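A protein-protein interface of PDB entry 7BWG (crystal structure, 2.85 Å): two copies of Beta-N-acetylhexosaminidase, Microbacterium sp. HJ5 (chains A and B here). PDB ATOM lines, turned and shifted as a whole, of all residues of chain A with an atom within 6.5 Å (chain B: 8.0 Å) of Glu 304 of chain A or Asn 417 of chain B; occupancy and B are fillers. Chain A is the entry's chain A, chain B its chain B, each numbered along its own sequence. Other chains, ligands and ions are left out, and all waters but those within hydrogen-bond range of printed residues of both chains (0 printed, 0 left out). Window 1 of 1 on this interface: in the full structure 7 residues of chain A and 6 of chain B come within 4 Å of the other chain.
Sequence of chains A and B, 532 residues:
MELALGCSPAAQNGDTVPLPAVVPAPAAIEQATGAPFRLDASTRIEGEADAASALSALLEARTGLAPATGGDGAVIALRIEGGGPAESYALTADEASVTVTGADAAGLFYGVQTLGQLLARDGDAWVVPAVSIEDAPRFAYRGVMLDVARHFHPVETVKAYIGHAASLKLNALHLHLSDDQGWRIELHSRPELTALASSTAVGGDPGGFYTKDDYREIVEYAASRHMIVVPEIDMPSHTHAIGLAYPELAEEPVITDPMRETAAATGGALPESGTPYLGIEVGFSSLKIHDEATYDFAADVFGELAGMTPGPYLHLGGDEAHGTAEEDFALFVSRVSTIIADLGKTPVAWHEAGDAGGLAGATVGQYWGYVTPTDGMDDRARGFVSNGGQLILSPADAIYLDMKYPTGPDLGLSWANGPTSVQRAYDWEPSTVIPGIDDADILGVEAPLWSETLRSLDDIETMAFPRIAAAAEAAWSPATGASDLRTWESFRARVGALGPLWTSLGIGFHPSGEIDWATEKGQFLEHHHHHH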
ATOM      1  N   GLU A 186     -36.162  -9.036  25.067  1.00  0.00           N
ATOM      2  CA  GLU A 186     -35.589  -8.626  23.789  1.00  0.00           C
ATOM      3  C   GLU A 186     -34.154  -8.162  23.999  1.00  0.00           C
ATOM      4  O   GLU A 186     -33.914  -7.079  24.544  1.00  0.00           O
ATOM      5  CB  GLU A 186     -36.429  -7.522  23.152  1.00  0.00           C
ATOM      6  CG  GLU A 186     -35.869  -6.997  21.838  1.00  0.00           C
ATOM      7  CD  GLU A 186     -36.807  -6.024  21.151  1.00  0.00           C
ATOM      8  OE1 GLU A 186     -36.693  -4.805  21.402  1.00  0.00           O
ATOM      9  OE2 GLU A 186     -37.660  -6.477  20.360  1.00  0.00           O
ATOM     10  N   LEU A 187     -33.203  -8.979  23.563  1.00  0.00           N
ATOM     11  CA  LEU A 187     -31.799  -8.605  23.525  1.00  0.00           C
ATOM     12  C   LEU A 187     -31.396  -8.281  22.092  1.00  0.00           C
ATOM     13  O   LEU A 187     -31.944  -8.831  21.135  1.00  0.00           O
ATOM     14  CB  LEU A 187     -30.914  -9.725  24.076  1.00  0.00           C
ATOM     15  N   HIS A 188     -30.433  -7.368  21.953  1.00  0.00           N
ATOM     16  CA  HIS A 188     -29.917  -6.994  20.646  1.00  0.00           C
ATOM     17  C   HIS A 188     -28.511  -7.512  20.378  1.00  0.00           C
ATOM     18  O   HIS A 188     -28.123  -7.617  19.211  1.00  0.00           O
ATOM     19  CB  HIS A 188     -29.939  -5.467  20.479  1.00  0.00           C
ATOM     20  CG  HIS A 188     -31.321  -4.890  20.432  1.00  0.00           C
ATOM     21  ND1 HIS A 188     -31.562  -3.533  20.377  1.00  0.00           N
ATOM     22  CD2 HIS A 188     -32.536  -5.487  20.433  1.00  0.00           C
ATOM     23  CE1 HIS A 188     -32.865  -3.320  20.346  1.00  0.00           C
ATOM     24  NE2 HIS A 188     -33.479  -4.489  20.379  1.00  0.00           N
ATOM     25  N   SER A 189     -27.743  -7.835  21.422  1.00  0.00           N
ATOM     26  CA  SER A 189     -26.491  -8.554  21.218  1.00  0.00           C
ATOM     27  C   SER A 189     -26.749  -9.986  20.769  1.00  0.00           C
ATOM     28  O   SER A 189     -25.925 -10.574  20.059  1.00  0.00           O
ATOM     29  CB  SER A 189     -25.657  -8.534  22.498  1.00  0.00           C
ATOM     30  OG  SER A 189     -26.367  -9.113  23.579  1.00  0.00           O
ATOM     31  N   ARG A 190     -27.883 -10.561  21.177  1.00  0.00           N
ATOM     32  CA  ARG A 190     -28.360 -11.854  20.697  1.00  0.00           C
ATOM     33  C   ARG A 190     -29.766 -11.627  20.155  1.00  0.00           C
ATOM     34  O   ARG A 190     -30.760 -12.000  20.798  1.00  0.00           O
ATOM     35  CB  ARG A 190     -28.343 -12.908  21.804  1.00  0.00           C
ATOM     36  CG  ARG A 190     -26.950 -13.295  22.272  1.00  0.00           C
ATOM     37  N   LYS A 212     -37.406  -4.377  24.806  1.00  0.00           N
ATOM     38  CA  LYS A 212     -36.655  -3.523  25.718  1.00  0.00           C
ATOM     39  C   LYS A 212     -37.494  -2.329  26.143  1.00  0.00           C
ATOM     40  O   LYS A 212     -37.475  -1.930  27.311  1.00  0.00           O
ATOM     41  CB  LYS A 212     -35.351  -3.066  25.059  1.00  0.00           C
ATOM     42  N   ALA A 299     -22.345 -14.110  28.627  1.00  0.00           N
ATOM     43  CA  ALA A 299     -21.821 -12.789  28.961  1.00  0.00           C
ATOM     44  C   ALA A 299     -22.537 -11.698  28.175  1.00  0.00           C
ATOM     45  O   ALA A 299     -22.832 -10.626  28.718  1.00  0.00           O
ATOM     46  CB  ALA A 299     -20.317 -12.737  28.704  1.00  0.00           C
ATOM     47  N   ASP A 300     -22.826 -11.954  26.897  1.00  0.00           N
ATOM     48  CA  ASP A 300     -23.519 -10.962  26.082  1.00  0.00           C
ATOM     49  C   ASP A 300     -24.950 -10.753  26.562  1.00  0.00           C
ATOM     50  O   ASP A 300     -25.424  -9.615  26.640  1.00  0.00           O
ATOM     51  CB  ASP A 300     -23.502 -11.387  24.614  1.00  0.00           C
ATOM     52  N   VAL A 301     -25.651 -11.840  26.889  1.00  0.00           N
ATOM     53  CA  VAL A 301     -27.037 -11.723  27.330  1.00  0.00           C
ATOM     54  C   VAL A 301     -27.104 -11.094  28.716  1.00  0.00           C
ATOM     55  O   VAL A 301     -27.882 -10.163  28.955  1.00  0.00           O
ATOM     56  CB  VAL A 301     -27.728 -13.097  27.296  1.00  0.00           C
ATOM     57  CG1 VAL A 301     -29.118 -13.003  27.898  1.00  0.00           C
ATOM     58  CG2 VAL A 301     -27.798 -13.613  25.870  1.00  0.00           C
ATOM     59  N   PHE A 302     -26.286 -11.588  29.648  1.00  0.00           N
ATOM     60  CA  PHE A 302     -26.309 -11.046  31.003  1.00  0.00           C
ATOM     61  C   PHE A 302     -25.724  -9.641  31.060  1.00  0.00           C
ATOM     62  O   PHE A 302     -26.145  -8.831  31.894  1.00  0.00           O
ATOM     63  CB  PHE A 302     -25.561 -11.979  31.956  1.00  0.00           C
ATOM     64  CG  PHE A 302     -26.412 -13.086  32.510  1.00  0.00           C
ATOM     65  CD1 PHE A 302     -27.619 -12.806  33.127  1.00  0.00           C
ATOM     66  CD2 PHE A 302     -26.009 -14.409  32.405  1.00  0.00           C
ATOM     67  CE1 PHE A 302     -28.408 -13.821  33.635  1.00  0.00           C
ATOM     68  CE2 PHE A 302     -26.795 -15.430  32.911  1.00  0.00           C
ATOM     69  CZ  PHE A 302     -27.995 -15.135  33.527  1.00  0.00           C
ATOM     70  N   GLY A 303     -24.761  -9.332  30.190  1.00  0.00           N
ATOM     71  CA  GLY A 303     -24.250  -7.973  30.128  1.00  0.00           C
ATOM     72  C   GLY A 303     -25.292  -6.990  29.631  1.00  0.00           C
ATOM     73  O   GLY A 303     -25.450  -5.901  30.191  1.00  0.00           O
ATOM     74  N   GLU A 304     -26.022  -7.360  28.576  1.00  0.00           N
ATOM     75  CA  GLU A 304     -27.105  -6.511  28.094  1.00  0.00           C
ATOM     76  C   GLU A 304     -28.264  -6.489  29.080  1.00  0.00           C
ATOM     77  O   GLU A 304     -28.928  -5.459  29.246  1.00  0.00           O
ATOM     78  CB  GLU A 304     -27.573  -6.992  26.720  1.00  0.00           C
ATOM     79  CG  GLU A 304     -28.708  -6.176  26.127  1.00  0.00           C
ATOM     80  CD  GLU A 304     -28.660  -6.127  24.613  1.00  0.00           C
ATOM     81  OE1 GLU A 304     -29.735  -6.034  23.985  1.00  0.00           O
ATOM     82  OE2 GLU A 304     -27.545  -6.181  24.052  1.00  0.00           O
ATOM     83  N   LEU A 305     -28.519  -7.617  29.748  1.00  0.00           N
ATOM     84  CA  LEU A 305     -29.598  -7.679  30.728  1.00  0.00           C
ATOM     85  C   LEU A 305     -29.334  -6.729  31.889  1.00  0.00           C
ATOM     86  O   LEU A 305     -30.213  -5.956  32.284  1.00  0.00           O
ATOM     87  CB  LEU A 305     -29.768  -9.111  31.234  1.00  0.00           C
ATOM     88  CG  LEU A 305     -31.167  -9.542  31.679  1.00  0.00           C
ATOM     89  CD1 LEU A 305     -31.993  -9.966  30.479  1.00  0.00           C
ATOM     90  CD2 LEU A 305     -31.083 -10.669  32.696  1.00  0.00           C
ATOM     91  N   ALA A 306     -28.116  -6.767  32.440  1.00  0.00           N
ATOM     92  CA  ALA A 306     -27.793  -5.936  33.596  1.00  0.00           C
ATOM     93  C   ALA A 306     -27.990  -4.455  33.293  1.00  0.00           C
ATOM     94  O   ALA A 306     -28.392  -3.684  34.171  1.00  0.00           O
ATOM     95  CB  ALA A 306     -26.360  -6.201  34.050  1.00  0.00           C
ATOM     96  N   GLY A 307     -27.712  -4.040  32.055  1.00  0.00           N
ATOM     97  CA  GLY A 307     -27.913  -2.653  31.676  1.00  0.00           C
ATOM     98  C   GLY A 307     -29.362  -2.217  31.699  1.00  0.00           C
ATOM     99  O   GLY A 307     -29.639  -1.019  31.825  1.00  0.00           O
ATOM    100  N   MET A 308     -30.295  -3.160  31.588  1.00  0.00           N
ATOM    101  CA  MET A 308     -31.717  -2.850  31.573  1.00  0.00           C
ATOM    102  C   MET A 308     -32.355  -2.892  32.956  1.00  0.00           C
ATOM    103  O   MET A 308     -33.500  -2.451  33.103  1.00  0.00           O
ATOM    104  CB  MET A 308     -32.457  -3.823  30.648  1.00  0.00           C
ATOM    105  CG  MET A 308     -31.895  -3.894  29.238  1.00  0.00           C
ATOM    106  SD  MET A 308     -32.907  -4.898  28.133  1.00  0.00           S
ATOM    107  CE  MET A 308     -32.130  -6.501  28.314  1.00  0.00           C
ATOM    108  N   THR A 309     -31.656  -3.405  33.962  1.00  0.00           N
ATOM    109  CA  THR A 309     -32.221  -3.560  35.302  1.00  0.00           C
ATOM    110  C   THR A 309     -31.465  -2.700  36.301  1.00  0.00           C
ATOM    111  O   THR A 309     -30.300  -3.009  36.623  1.00  0.00           O
ATOM    112  CB  THR A 309     -32.183  -5.023  35.743  1.00  0.00           C
ATOM    113  OG1 THR A 309     -30.930  -5.302  36.378  1.00  0.00           O
ATOM    114  CG2 THR A 309     -32.344  -5.933  34.548  1.00  0.00           C
ATOM    115  N   LEU A 343     -20.044  -7.761  36.384  1.00  0.00           N
ATOM    116  CA  LEU A 343     -20.911  -6.756  35.786  1.00  0.00           C
ATOM    117  C   LEU A 343     -21.367  -5.701  36.785  1.00  0.00           C
ATOM    118  O   LEU A 343     -22.033  -4.740  36.386  1.00  0.00           O
ATOM    119  CB  LEU A 343     -22.138  -7.427  35.161  1.00  0.00           C
ATOM    120  CG  LEU A 343     -21.927  -8.095  33.803  1.00  0.00           C
ATOM    121  CD1 LEU A 343     -23.099  -9.000  33.455  1.00  0.00           C
ATOM    122  CD2 LEU A 343     -21.722  -7.043  32.734  1.00  0.00           C
ATOM    123  N   TRP B 368     -25.240   6.327  22.626  1.00  0.00           N
ATOM    124  CA  TRP B 368     -26.055   5.131  22.756  1.00  0.00           C
ATOM    125  C   TRP B 368     -25.409   3.952  22.030  1.00  0.00           C
ATOM    126  O   TRP B 368     -24.488   4.105  21.226  1.00  0.00           O
ATOM    127  CB  TRP B 368     -27.461   5.379  22.213  1.00  0.00           C
ATOM    128  N   GLY B 369     -25.920   2.758  22.323  1.00  0.00           N
ATOM    129  CA  GLY B 369     -25.368   1.551  21.738  1.00  0.00           C
ATOM    130  C   GLY B 369     -25.481   1.532  20.226  1.00  0.00           C
ATOM    131  O   GLY B 369     -26.305   2.217  19.620  1.00  0.00           O
ATOM    132  N   TYR B 370     -24.614   0.723  19.610  1.00  0.00           N
ATOM    133  CA  TYR B 370     -24.599   0.603  18.157  1.00  0.00           C
ATOM    134  C   TYR B 370     -25.886  -0.007  17.617  1.00  0.00           C
ATOM    135  O   TYR B 370     -26.257   0.269  16.468  1.00  0.00           O
ATOM    136  CB  TYR B 370     -23.388  -0.225  17.722  1.00  0.00           C
ATOM    137  N   VAL B 371     -26.587  -0.805  18.422  1.00  0.00           N
ATOM    138  CA  VAL B 371     -27.913  -1.297  18.065  1.00  0.00           C
ATOM    139  C   VAL B 371     -29.023  -0.386  18.595  1.00  0.00           C
ATOM    140  O   VAL B 371     -30.196  -0.773  18.580  1.00  0.00           O
ATOM    141  CB  VAL B 371     -28.121  -2.730  18.565  1.00  0.00           C
ATOM    142  N   THR B 372     -28.681   0.840  19.021  1.00  0.00           N
ATOM    143  CA  THR B 372     -29.534   1.851  19.659  1.00  0.00           C
ATOM    144  C   THR B 372     -30.703   1.258  20.447  1.00  0.00           C
ATOM    145  O   THR B 372     -31.846   1.268  19.972  1.00  0.00           O
ATOM    146  CB  THR B 372     -30.050   2.868  18.626  1.00  0.00           C
ATOM    147  OG1 THR B 372     -31.130   3.623  19.192  1.00  0.00           O
ATOM    148  CG2 THR B 372     -30.525   2.214  17.327  1.00  0.00           C
ATOM    149  N   PRO B 373     -30.453   0.729  21.663  1.00  0.00           N
ATOM    150  CA  PRO B 373     -31.547   0.364  22.577  1.00  0.00           C
ATOM    151  C   PRO B 373     -32.089   1.606  23.259  1.00  0.00           C
ATOM    152  O   PRO B 373     -31.407   2.240  24.075  1.00  0.00           O
ATOM    153  CB  PRO B 373     -30.865  -0.592  23.567  1.00  0.00           C
ATOM    154  CG  PRO B 373     -29.447  -0.122  23.606  1.00  0.00           C
ATOM    155  CD  PRO B 373     -29.127   0.446  22.243  1.00  0.00           C
ATOM    156  N   ALA B 396     -21.631   3.597  22.951  1.00  0.00           N
ATOM    157  CA  ALA B 396     -21.115   3.182  24.253  1.00  0.00           C
ATOM    158  C   ALA B 396     -20.595   1.754  24.211  1.00  0.00           C
ATOM    159  O   ALA B 396     -19.460   1.481  24.620  1.00  0.00           O
ATOM    160  CB  ALA B 396     -22.200   3.322  25.321  1.00  0.00           C
ATOM    161  N   ASP B 397     -21.418   0.821  23.729  1.00  0.00           N
ATOM    162  CA  ASP B 397     -20.977  -0.566  23.653  1.00  0.00           C
ATOM    163  C   ASP B 397     -19.793  -0.724  22.710  1.00  0.00           C
ATOM    164  O   ASP B 397     -18.926  -1.575  22.939  1.00  0.00           O
ATOM    165  CB  ASP B 397     -22.137  -1.464  23.216  1.00  0.00           C
ATOM    166  CG  ASP B 397     -22.749  -1.030  21.900  1.00  0.00           C
ATOM    167  OD1 ASP B 397     -22.527   0.129  21.494  1.00  0.00           O
ATOM    168  OD2 ASP B 397     -23.451  -1.851  21.271  1.00  0.00           O
ATOM    169  N   ALA B 398     -19.716   0.102  21.668  1.00  0.00           N
ATOM    170  CA  ALA B 398     -18.663  -0.030  20.668  1.00  0.00           C
ATOM    171  C   ALA B 398     -17.415   0.770  21.033  1.00  0.00           C
ATOM    172  O   ALA B 398     -16.346   0.195  21.260  1.00  0.00           O
ATOM    173  CB  ALA B 398     -19.190   0.400  19.294  1.00  0.00           C
ATOM    174  N   MET B 403     -14.623   1.047  28.847  1.00  0.00           N
ATOM    175  CA  MET B 403     -15.285  -0.215  29.139  1.00  0.00           C
ATOM    176  C   MET B 403     -14.252  -1.315  29.339  1.00  0.00           C
ATOM    177  O   MET B 403     -13.267  -1.404  28.601  1.00  0.00           O
ATOM    178  CB  MET B 403     -16.250  -0.587  28.015  1.00  0.00           C
ATOM    179  CG  MET B 403     -17.583  -1.125  28.507  1.00  0.00           C
ATOM    180  SD  MET B 403     -18.452   0.049  29.566  1.00  0.00           S
ATOM    181  CE  MET B 403     -18.831   1.351  28.396  1.00  0.00           C
ATOM    182  N   LEU B 413     -15.016  -0.140  33.126  1.00  0.00           N
ATOM    183  CA  LEU B 413     -16.384  -0.328  33.583  1.00  0.00           C
ATOM    184  C   LEU B 413     -17.084  -1.318  32.662  1.00  0.00           C
ATOM    185  O   LEU B 413     -16.510  -1.808  31.685  1.00  0.00           O
ATOM    186  CB  LEU B 413     -17.140   1.006  33.638  1.00  0.00           C
ATOM    187  CG  LEU B 413     -16.582   2.046  34.611  1.00  0.00           C
ATOM    188  CD1 LEU B 413     -17.312   3.371  34.460  1.00  0.00           C
ATOM    189  CD2 LEU B 413     -16.670   1.538  36.043  1.00  0.00           C
ATOM    190  N   SER B 414     -18.349  -1.614  32.979  1.00  0.00           N
ATOM    191  CA  SER B 414     -19.118  -2.576  32.198  1.00  0.00           C
ATOM    192  C   SER B 414     -20.574  -2.153  32.034  1.00  0.00           C
ATOM    193  O   SER B 414     -21.419  -2.994  31.709  1.00  0.00           O
ATOM    194  CB  SER B 414     -19.060  -3.965  32.844  1.00  0.00           C
ATOM    195  OG  SER B 414     -19.570  -3.932  34.167  1.00  0.00           O
ATOM    196  N   TRP B 415     -20.885  -0.869  32.238  1.00  0.00           N
ATOM    197  CA  TRP B 415     -22.276  -0.436  32.302  1.00  0.00           C
ATOM    198  C   TRP B 415     -22.981  -0.490  30.954  1.00  0.00           C
ATOM    199  O   TRP B 415     -24.211  -0.385  30.916  1.00  0.00           O
ATOM    200  CB  TRP B 415     -22.361   0.984  32.869  1.00  0.00           C
ATOM    201  CG  TRP B 415     -21.742   2.034  31.993  1.00  0.00           C
ATOM    202  CD1 TRP B 415     -20.496   2.576  32.122  1.00  0.00           C
ATOM    203  CD2 TRP B 415     -22.343   2.678  30.860  1.00  0.00           C
ATOM    204  NE1 TRP B 415     -20.282   3.511  31.139  1.00  0.00           N
ATOM    205  CE2 TRP B 415     -21.401   3.592  30.352  1.00  0.00           C
ATOM    206  CE3 TRP B 415     -23.585   2.568  30.227  1.00  0.00           C
ATOM    207  CZ2 TRP B 415     -21.661   4.389  29.241  1.00  0.00           C
ATOM    208  CZ3 TRP B 415     -23.840   3.357  29.124  1.00  0.00           C
ATOM    209  CH2 TRP B 415     -22.883   4.258  28.643  1.00  0.00           C
ATOM    210  N   ALA B 416     -22.239  -0.628  29.854  1.00  0.00           N
ATOM    211  CA  ALA B 416     -22.849  -0.700  28.532  1.00  0.00           C
ATOM    212  C   ALA B 416     -23.711  -1.951  28.414  1.00  0.00           C
ATOM    213  O   ALA B 416     -24.855  -1.974  28.878  1.00  0.00           O
ATOM    214  CB  ALA B 416     -21.776  -0.683  27.441  1.00  0.00           C
ATOM    215  N   ASN B 417     -23.173  -2.992  27.788  1.00  0.00           N
ATOM    216  CA  ASN B 417     -23.791  -4.312  27.766  1.00  0.00           C
ATOM    217  C   ASN B 417     -22.738  -5.373  28.042  1.00  0.00           C
ATOM    218  O   ASN B 417     -22.584  -6.353  27.310  1.00  0.00           O
ATOM    219  CB  ASN B 417     -24.506  -4.563  26.444  1.00  0.00           C
ATOM    220  CG  ASN B 417     -25.687  -3.633  26.237  1.00  0.00           C
ATOM    221  OD1 ASN B 417     -26.462  -3.378  27.161  1.00  0.00           O
ATOM    222  ND2 ASN B 417     -25.832  -3.123  25.020  1.00  0.00           N
ATOM    223  N   GLY B 418     -21.996  -5.174  29.129  1.00  0.00           N
ATOM    224  CA  GLY B 418     -20.890  -6.029  29.473  1.00  0.00           C
ATOM    225  C   GLY B 418     -19.570  -5.416  29.058  1.00  0.00           C
ATOM    226  O   GLY B 418     -19.501  -4.255  28.641  1.00  0.00           O
ATOM    227  N   PRO B 419     -18.489  -6.182  29.186  1.00  0.00           N
ATOM    228  CA  PRO B 419     -17.200  -5.725  28.661  1.00  0.00           C
ATOM    229  C   PRO B 419     -17.259  -5.554  27.151  1.00  0.00           C
ATOM    230  O   PRO B 419     -18.117  -6.114  26.465  1.00  0.00           O
ATOM    231  CB  PRO B 419     -16.233  -6.845  29.060  1.00  0.00           C
ATOM    232  CG  PRO B 419     -16.899  -7.532  30.206  1.00  0.00           C
ATOM    233  CD  PRO B 419     -18.369  -7.444  29.933  1.00  0.00           C
ATOM    234  N   THR B 420     -16.328  -4.758  26.633  1.00  0.00           N
ATOM    235  CA  THR B 420     -16.251  -4.457  25.208  1.00  0.00           C
ATOM    236  C   THR B 420     -15.031  -5.159  24.626  1.00  0.00           C
ATOM    237  O   THR B 420     -13.890  -4.792  24.932  1.00  0.00           O
ATOM    238  CB  THR B 420     -16.180  -2.952  24.965  1.00  0.00           C
ATOM    239  OG1 THR B 420     -17.444  -2.354  25.280  1.00  0.00           O
ATOM    240  CG2 THR B 420     -15.842  -2.664  23.508  1.00  0.00           C
ATOM    241  N   ARG B 424     -15.986  -5.901  18.945  1.00  0.00           N
ATOM    242  CA  ARG B 424     -17.206  -5.104  19.020  1.00  0.00           C
ATOM    243  C   ARG B 424     -16.913  -3.613  18.887  1.00  0.00           C
ATOM    244  O   ARG B 424     -17.742  -2.865  18.357  1.00  0.00           O
ATOM    245  CB  ARG B 424     -17.945  -5.406  20.325  1.00  0.00           C
ATOM    246  CG  ARG B 424     -19.053  -4.430  20.671  1.00  0.00           C
ATOM    247  CD  ARG B 424     -19.404  -4.508  22.141  1.00  0.00           C
ATOM    248  NE  ARG B 424     -20.804  -4.858  22.361  1.00  0.00           N
ATOM    249  CZ  ARG B 424     -21.359  -4.977  23.561  1.00  0.00           C
ATOM    250  NH1 ARG B 424     -20.631  -4.775  24.652  1.00  0.00           N
ATOM    251  NH2 ARG B 424     -22.641  -5.298  23.674  1.00  0.00           N
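Of chain B, only Asn 417 (3.3 Å) comes within 4 Å of Glu 304 of chain A. Asn 417 of chain B touches two residues of chain A. Of the printed residues of chain B, Gly 303 of chain A touches Asn 417 and Gly 418. Of the printed residues of chain B, His 188 of chain A touches Val 371 (3.6 Å). Of the printed residues of chain A, Ser 414 of chain B touches Leu 343. Of the printed residues of chain B, Leu 343 of chain A touches Ser 414 (3.4 Å) and Gly 418 (3.5 Å). The nearest residue of chain A that does not touch Asn 417 of chain B is Asp 300 of chain A (4.4 Å). The nearest printed residue of chain B that does not touch His 188 of chain A is Pro 373 of chain B (4.4 Å).
The side-chain carboxylate of Glu 186 of chain A sits at hydrogen-bond distance from a ring nitrogen (NE2) of His 188 of chain A (3.4 Å). OE1 of Glu 304 of chain A lies within hydrogen-bond range of N of His 188 of chain A, 2.5 Å away. N of Ser 189 of chain A is in hydrogen-bond range of OE2 of Glu 304 of chain A, at 3.1 Å. The backbone NH of Ser 414 of chain B lies close to the side-chain sulfur of Met 403 of chain B, at 3.8 Å.
Hydrophobic or aromatic side chains of chain A that line the printed part of chain B: His 188 and Leu 343. Of the 19 printed residues of chain B, 4 touch a printed residue of chain A. Hydrophobic or aromatic side chains of chain B that line the printed part of chain A: Val 371.
No position is printed for both chains. Of the 6 pairs that touch across the chains among the printed residues, none has its exchanged pair printed and touching as well.
O of Leu 343 of chain A lies within hydrogen-bond range of OG of Ser 414 of chain B.
Among the printed residues, merely in contact across the chains: Glu 304 of chain A with Asn 417 of chain B (3.3 Å), Gly 303 of chain A with Asn 417 of chain B (3.3 Å), Leu 343 of chain A with Gly 418 of chain B (3.5 Å), His 188 of chain A with Val 371 of chain B (3.6 Å) and Gly 303 of chain A with Gly 418 of chain B (3.7 Å).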
